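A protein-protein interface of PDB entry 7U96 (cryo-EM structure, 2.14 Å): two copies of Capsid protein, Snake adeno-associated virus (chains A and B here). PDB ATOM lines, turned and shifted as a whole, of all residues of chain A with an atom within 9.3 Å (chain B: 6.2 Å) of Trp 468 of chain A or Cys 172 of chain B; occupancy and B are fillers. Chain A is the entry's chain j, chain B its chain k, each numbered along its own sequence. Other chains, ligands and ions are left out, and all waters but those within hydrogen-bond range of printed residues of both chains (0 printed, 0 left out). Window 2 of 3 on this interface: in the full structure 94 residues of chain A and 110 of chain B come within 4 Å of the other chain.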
ATOM      1  N   SER A 465      32.395 -21.445  11.404  1.00  0.00           N
ATOM      2  CA  SER A 465      31.087 -21.963  11.831  1.00  0.00           C
ATOM      3  C   SER A 465      31.080 -23.460  12.126  1.00  0.00           C
ATOM      4  O   SER A 465      31.685 -24.259  11.412  1.00  0.00           O
ATOM      5  CB  SER A 465      30.030 -21.670  10.773  1.00  0.00           C
ATOM      6  OG  SER A 465      30.326 -22.352   9.565  1.00  0.00           O
ATOM      7  N   LYS A 466      30.385 -23.832  13.201  1.00  0.00           N
ATOM      8  CA  LYS A 466      30.312 -25.203  13.689  1.00  0.00           C
ATOM      9  C   LYS A 466      29.038 -25.968  13.325  1.00  0.00           C
ATOM     10  O   LYS A 466      28.802 -27.021  13.914  1.00  0.00           O
ATOM     11  CB  LYS A 466      30.510 -25.250  15.196  1.00  0.00           C
ATOM     12  CG  LYS A 466      31.935 -24.988  15.616  1.00  0.00           C
ATOM     13  CD  LYS A 466      32.094 -25.304  17.081  1.00  0.00           C
ATOM     14  CE  LYS A 466      32.090 -26.801  17.358  1.00  0.00           C
ATOM     15  NZ  LYS A 466      33.373 -27.481  17.004  1.00  0.00           N
ATOM     16  N   ARG A 467      28.178 -25.455  12.454  1.00  0.00           N
ATOM     17  CA  ARG A 467      27.010 -26.237  12.057  1.00  0.00           C
ATOM     18  C   ARG A 467      27.417 -27.551  11.401  1.00  0.00           C
ATOM     19  O   ARG A 467      28.485 -27.666  10.800  1.00  0.00           O
ATOM     20  CB  ARG A 467      26.107 -25.444  11.111  1.00  0.00           C
ATOM     21  CG  ARG A 467      26.746 -25.012   9.823  1.00  0.00           C
ATOM     22  CD  ARG A 467      25.821 -24.124   9.006  1.00  0.00           C
ATOM     23  NE  ARG A 467      24.812 -24.809   8.212  1.00  0.00           N
ATOM     24  CZ  ARG A 467      23.770 -24.192   7.667  1.00  0.00           C
ATOM     25  NH1 ARG A 467      23.573 -22.908   7.896  1.00  0.00           N
ATOM     26  NH2 ARG A 467      22.899 -24.859   6.938  1.00  0.00           N
ATOM     27  N   TRP A 468      26.551 -28.554  11.545  1.00  0.00           N
ATOM     28  CA  TRP A 468      26.842 -29.893  11.048  1.00  0.00           C
ATOM     29  C   TRP A 468      26.587 -30.010   9.549  1.00  0.00           C
ATOM     30  O   TRP A 468      27.407 -30.568   8.814  1.00  0.00           O
ATOM     31  CB  TRP A 468      25.999 -30.916  11.810  1.00  0.00           C
ATOM     32  CG  TRP A 468      26.205 -32.313  11.360  1.00  0.00           C
ATOM     33  CD1 TRP A 468      25.437 -33.005  10.487  1.00  0.00           C
ATOM     34  CD2 TRP A 468      27.230 -33.207  11.786  1.00  0.00           C
ATOM     35  NE1 TRP A 468      25.926 -34.263  10.321  1.00  0.00           N
ATOM     36  CE2 TRP A 468      27.030 -34.415  11.110  1.00  0.00           C
ATOM     37  CE3 TRP A 468      28.303 -33.098  12.669  1.00  0.00           C
ATOM     38  CZ2 TRP A 468      27.858 -35.509  11.286  1.00  0.00           C
ATOM     39  CZ3 TRP A 468      29.120 -34.183  12.844  1.00  0.00           C
ATOM     40  CH2 TRP A 468      28.898 -35.373  12.154  1.00  0.00           C
ATOM     41  N   ASN A 469      25.451 -29.516   9.082  1.00  0.00           N
ATOM     42  CA  ASN A 469      25.060 -29.670   7.692  1.00  0.00           C
ATOM     43  C   ASN A 469      25.772 -28.663   6.790  1.00  0.00           C
ATOM     44  O   ASN A 469      26.255 -27.630   7.251  1.00  0.00           O
ATOM     45  CB  ASN A 469      23.549 -29.526   7.552  1.00  0.00           C
ATOM     46  CG  ASN A 469      23.029 -28.229   8.121  1.00  0.00           C
ATOM     47  OD1 ASN A 469      23.620 -27.653   9.025  1.00  0.00           O
ATOM     48  ND2 ASN A 469      21.948 -27.736   7.557  1.00  0.00           N
ATOM     49  N   PRO A 470      25.860 -28.952   5.494  1.00  0.00           N
ATOM     50  CA  PRO A 470      26.546 -28.036   4.578  1.00  0.00           C
ATOM     51  C   PRO A 470      25.786 -26.735   4.363  1.00  0.00           C
ATOM     52  O   PRO A 470      24.604 -26.615   4.678  1.00  0.00           O
ATOM     53  CB  PRO A 470      26.653 -28.850   3.287  1.00  0.00           C
ATOM     54  CG  PRO A 470      25.581 -29.849   3.388  1.00  0.00           C
ATOM     55  CD  PRO A 470      25.479 -30.203   4.820  1.00  0.00           C
ATOM     56  N   GLU A 471      26.487 -25.763   3.796  1.00  0.00           N
ATOM     57  CA  GLU A 471      26.011 -24.402   3.604  1.00  0.00           C
ATOM     58  C   GLU A 471      25.885 -24.068   2.126  1.00  0.00           C
ATOM     59  O   GLU A 471      26.414 -24.764   1.261  1.00  0.00           O
ATOM     60  CB  GLU A 471      26.952 -23.394   4.256  1.00  0.00           C
ATOM     61  CG  GLU A 471      26.928 -23.387   5.749  1.00  0.00           C
ATOM     62  CD  GLU A 471      27.846 -22.335   6.310  1.00  0.00           C
ATOM     63  OE1 GLU A 471      28.614 -21.760   5.522  1.00  0.00           O
ATOM     64  OE2 GLU A 471      27.803 -22.075   7.527  1.00  0.00           O
ATOM     65  N   TYR B  32      17.989 -36.761  19.115  1.00  0.00           N
ATOM     66  CA  TYR B  32      17.624 -35.480  18.537  1.00  0.00           C
ATOM     67  C   TYR B  32      16.283 -35.637  17.847  1.00  0.00           C
ATOM     68  O   TYR B  32      15.911 -36.739  17.447  1.00  0.00           O
ATOM     69  CB  TYR B  32      18.670 -35.015  17.524  1.00  0.00           C
ATOM     70  CG  TYR B  32      19.984 -34.615  18.125  1.00  0.00           C
ATOM     71  CD1 TYR B  32      20.260 -33.291  18.405  1.00  0.00           C
ATOM     72  CD2 TYR B  32      20.932 -35.563  18.450  1.00  0.00           C
ATOM     73  CE1 TYR B  32      21.453 -32.921  18.954  1.00  0.00           C
ATOM     74  CE2 TYR B  32      22.121 -35.207  19.012  1.00  0.00           C
ATOM     75  CZ  TYR B  32      22.381 -33.884  19.261  1.00  0.00           C
ATOM     76  OH  TYR B  32      23.574 -33.521  19.821  1.00  0.00           O
ATOM     77  N   TRP B  56      20.508 -32.780  25.398  1.00  0.00           N
ATOM     78  CA  TRP B  56      21.292 -32.091  26.415  1.00  0.00           C
ATOM     79  C   TRP B  56      20.427 -31.193  27.312  1.00  0.00           C
ATOM     80  O   TRP B  56      19.236 -30.982  27.079  1.00  0.00           O
ATOM     81  CB  TRP B  56      22.365 -31.249  25.729  1.00  0.00           C
ATOM     82  CG  TRP B  56      23.452 -32.020  25.065  1.00  0.00           C
ATOM     83  CD1 TRP B  56      23.392 -32.642  23.859  1.00  0.00           C
ATOM     84  CD2 TRP B  56      24.799 -32.160  25.516  1.00  0.00           C
ATOM     85  NE1 TRP B  56      24.597 -33.200  23.552  1.00  0.00           N
ATOM     86  CE2 TRP B  56      25.481 -32.921  24.555  1.00  0.00           C
ATOM     87  CE3 TRP B  56      25.492 -31.725  26.644  1.00  0.00           C
ATOM     88  CZ2 TRP B  56      26.813 -33.274  24.691  1.00  0.00           C
ATOM     89  CZ3 TRP B  56      26.819 -32.062  26.767  1.00  0.00           C
ATOM     90  CH2 TRP B  56      27.470 -32.819  25.793  1.00  0.00           C
ATOM     91  N   LEU B 127      26.765 -21.944  19.536  1.00  0.00           N
ATOM     92  CA  LEU B 127      25.394 -22.407  19.556  1.00  0.00           C
ATOM     93  C   LEU B 127      24.427 -21.235  19.603  1.00  0.00           C
ATOM     94  O   LEU B 127      24.778 -20.148  20.057  1.00  0.00           O
ATOM     95  CB  LEU B 127      25.176 -23.323  20.748  1.00  0.00           C
ATOM     96  CG  LEU B 127      25.955 -24.629  20.669  1.00  0.00           C
ATOM     97  CD1 LEU B 127      25.839 -25.396  21.959  1.00  0.00           C
ATOM     98  CD2 LEU B 127      25.437 -25.458  19.514  1.00  0.00           C
ATOM     99  N   PHE B 170      21.458 -27.266  11.510  1.00  0.00           N
ATOM    100  CA  PHE B 170      21.436 -28.354  12.475  1.00  0.00           C
ATOM    101  C   PHE B 170      22.770 -28.403  13.203  1.00  0.00           C
ATOM    102  O   PHE B 170      23.827 -28.360  12.571  1.00  0.00           O
ATOM    103  CB  PHE B 170      21.151 -29.690  11.794  1.00  0.00           C
ATOM    104  CG  PHE B 170      21.300 -30.868  12.701  1.00  0.00           C
ATOM    105  CD1 PHE B 170      20.349 -31.143  13.657  1.00  0.00           C
ATOM    106  CD2 PHE B 170      22.385 -31.711  12.587  1.00  0.00           C
ATOM    107  CE1 PHE B 170      20.484 -32.219  14.492  1.00  0.00           C
ATOM    108  CE2 PHE B 170      22.525 -32.793  13.421  1.00  0.00           C
ATOM    109  CZ  PHE B 170      21.572 -33.047  14.376  1.00  0.00           C
ATOM    110  N   TYR B 171      22.721 -28.491  14.525  1.00  0.00           N
ATOM    111  CA  TYR B 171      23.921 -28.528  15.345  1.00  0.00           C
ATOM    112  C   TYR B 171      24.009 -29.865  16.061  1.00  0.00           C
ATOM    113  O   TYR B 171      23.020 -30.337  16.627  1.00  0.00           O
ATOM    114  CB  TYR B 171      23.930 -27.385  16.355  1.00  0.00           C
ATOM    115  CG  TYR B 171      23.882 -26.027  15.716  1.00  0.00           C
ATOM    116  CD1 TYR B 171      25.040 -25.400  15.286  1.00  0.00           C
ATOM    117  CD2 TYR B 171      22.678 -25.373  15.532  1.00  0.00           C
ATOM    118  CE1 TYR B 171      24.996 -24.163  14.695  1.00  0.00           C
ATOM    119  CE2 TYR B 171      22.623 -24.143  14.949  1.00  0.00           C
ATOM    120  CZ  TYR B 171      23.783 -23.537  14.532  1.00  0.00           C
ATOM    121  OH  TYR B 171      23.720 -22.300  13.950  1.00  0.00           O
ATOM    122  N   CYS B 172      25.183 -30.476  16.022  1.00  0.00           N
ATOM    123  CA  CYS B 172      25.492 -31.672  16.793  1.00  0.00           C
ATOM    124  C   CYS B 172      26.311 -31.254  18.001  1.00  0.00           C
ATOM    125  O   CYS B 172      27.402 -30.700  17.850  1.00  0.00           O
ATOM    126  CB  CYS B 172      26.262 -32.687  15.952  1.00  0.00           C
ATOM    127  SG  CYS B 172      26.745 -34.177  16.832  1.00  0.00           S
ATOM    128  N   LEU B 173      25.796 -31.519  19.193  1.00  0.00           N
ATOM    129  CA  LEU B 173      26.506 -31.059  20.375  1.00  0.00           C
ATOM    130  C   LEU B 173      27.626 -32.008  20.765  1.00  0.00           C
ATOM    131  O   LEU B 173      28.511 -31.629  21.534  1.00  0.00           O
ATOM    132  CB  LEU B 173      25.529 -30.846  21.525  1.00  0.00           C
ATOM    133  CG  LEU B 173      24.866 -29.465  21.555  1.00  0.00           C
ATOM    134  CD1 LEU B 173      24.005 -29.211  20.328  1.00  0.00           C
ATOM    135  CD2 LEU B 173      24.043 -29.315  22.800  1.00  0.00           C
ATOM    136  N   GLU B 174      27.628 -33.228  20.233  1.00  0.00           N
ATOM    137  CA  GLU B 174      28.763 -34.115  20.451  1.00  0.00           C
ATOM    138  C   GLU B 174      29.970 -33.692  19.638  1.00  0.00           C
ATOM    139  O   GLU B 174      31.052 -34.246  19.826  1.00  0.00           O
ATOM    140  CB  GLU B 174      28.378 -35.558  20.131  1.00  0.00           C
ATOM    141  CG  GLU B 174      27.402 -36.146  21.133  1.00  0.00           C
ATOM    142  CD  GLU B 174      25.990 -35.664  20.919  1.00  0.00           C
ATOM    143  OE1 GLU B 174      25.766 -34.902  19.964  1.00  0.00           O
ATOM    144  OE2 GLU B 174      25.110 -36.009  21.726  1.00  0.00           O
ATOM    145  N   TYR B 175      29.811 -32.706  18.761  1.00  0.00           N
ATOM    146  CA  TYR B 175      30.922 -32.240  17.946  1.00  0.00           C
ATOM    147  C   TYR B 175      31.767 -31.225  18.707  1.00  0.00           C
ATOM    148  O   TYR B 175      32.771 -30.726  18.193  1.00  0.00           O
ATOM    149  CB  TYR B 175      30.362 -31.665  16.643  1.00  0.00           C
ATOM    150  CG  TYR B 175      31.364 -31.138  15.647  1.00  0.00           C
ATOM    151  CD1 TYR B 175      32.100 -31.998  14.853  1.00  0.00           C
ATOM    152  CD2 TYR B 175      31.543 -29.775  15.476  1.00  0.00           C
ATOM    153  CE1 TYR B 175      33.004 -31.523  13.932  1.00  0.00           C
ATOM    154  CE2 TYR B 175      32.446 -29.285  14.559  1.00  0.00           C
ATOM    155  CZ  TYR B 175      33.177 -30.164  13.789  1.00  0.00           C
ATOM    156  OH  TYR B 175      34.079 -29.675  12.875  1.00  0.00           O
ATOM    157  N   PHE B 176      31.364 -30.891  19.927  1.00  0.00           N
ATOM    158  CA  PHE B 176      32.153 -30.023  20.786  1.00  0.00           C
ATOM    159  C   PHE B 176      33.041 -30.843  21.718  1.00  0.00           C
ATOM    160  O   PHE B 176      32.679 -31.947  22.118  1.00  0.00           O
ATOM    161  CB  PHE B 176      31.237 -29.141  21.618  1.00  0.00           C
ATOM    162  CG  PHE B 176      30.443 -28.174  20.814  1.00  0.00           C
ATOM    163  CD1 PHE B 176      30.857 -26.873  20.674  1.00  0.00           C
ATOM    164  CD2 PHE B 176      29.314 -28.583  20.142  1.00  0.00           C
ATOM    165  CE1 PHE B 176      30.123 -25.987  19.930  1.00  0.00           C
ATOM    166  CE2 PHE B 176      28.593 -27.709  19.389  1.00  0.00           C
ATOM    167  CZ  PHE B 176      28.997 -26.412  19.275  1.00  0.00           C
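The side-chain carboxylate of Glu 174 of chain B is in hydrogen-bond range of the side-chain sulfur of Cys 172 of chain B (3.4 Å).
O of Pro 470 of chain A is in hydrogen-bond range of NH2 of Arg 467 of chain A (3.3 Å).
NH2 of Arg 467 of chain A lies close to ND2 of Asn 469 of chain A, 3.1 Å away.
Of chain B, only Phe 170 (2.9 Å) and Cys 172 (3.9 Å) come within 4 Å of Trp 468 of chain A.
Of chain A, only Trp 468 comes within 4 Å of Cys 172 of chain B.
Of the printed residues of chain A, Phe 176 of chain B touches Lys 466 (3.3 Å).
Of the printed residues of chain B, Asn 469 of chain A touches Phe 170.
Of the printed residues of chain A, Phe 170 of chain B touches Arg 467 (3.9 Å), Trp 468 (2.9 Å) and Asn 469 (3.3 Å).
Printed residues of chain A within 4 Å of Tyr 171 of chain B: Arg 467.
Leu 173 of chain B touches none of the printed residues of chain A.
Tyr 32 of chain B touches none of the printed residues of chain A.
The nearest residue of chain B that does not touch Trp 468 of chain A is Tyr 175 of chain B (4.2 Å).
The nearest residue of chain A that does not touch Cys 172 of chain B is Lys 466 of chain A (5.4 Å).
The nearest printed residue of chain B that does not touch Lys 466 of chain A is Tyr 171 of chain B (4.3 Å).
Lys 466 of chain A touches Tyr 175 of chain B (NZ to CE2, 3.2 Å).
Phe 176 of chain B touches Lys 466 of chain A.
O of Phe 170 of chain B touches CA of Arg 467 of chain A, at 3.9 Å.
CA of Arg 467 of chain A touches CD1 of Tyr 171 of chain B (3.9 Å).
CE3 of Trp 468 of chain A touches CB of Cys 172 of chain B (3.9 Å).
The backbone NH of Trp 468 of chain A lies within hydrogen-bond range of the backbone carbonyl oxygen of Phe 170 of chain B, 2.9 Å away.
OD1 of Asn 469 of chain A sits at hydrogen-bond distance from N of Phe 170 of chain B, at 3.3 Å.
Hydrophobic or aromatic side chains of chain A within 4 Å of the printed part of chain B: Trp 468.
Of the 10 printed residues of chain B, 5 touch a printed residue of chain A.
Printed residues of chain B that touch a printed residue of chain A: Phe 170, Tyr 171, Cys 172, Tyr 175 and Phe 176.
Hydrophobic or aromatic side chains of chain B within 4 Å of the printed part of chain A: Phe 170, Tyr 171, Tyr 175 and Phe 176.
Among the printed residues, 7 pairs touch across the chains.
No position is printed for both chains.
Of the 7 pairs that touch across the chains among the printed residues, none has its exchanged pair printed and touching as well.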
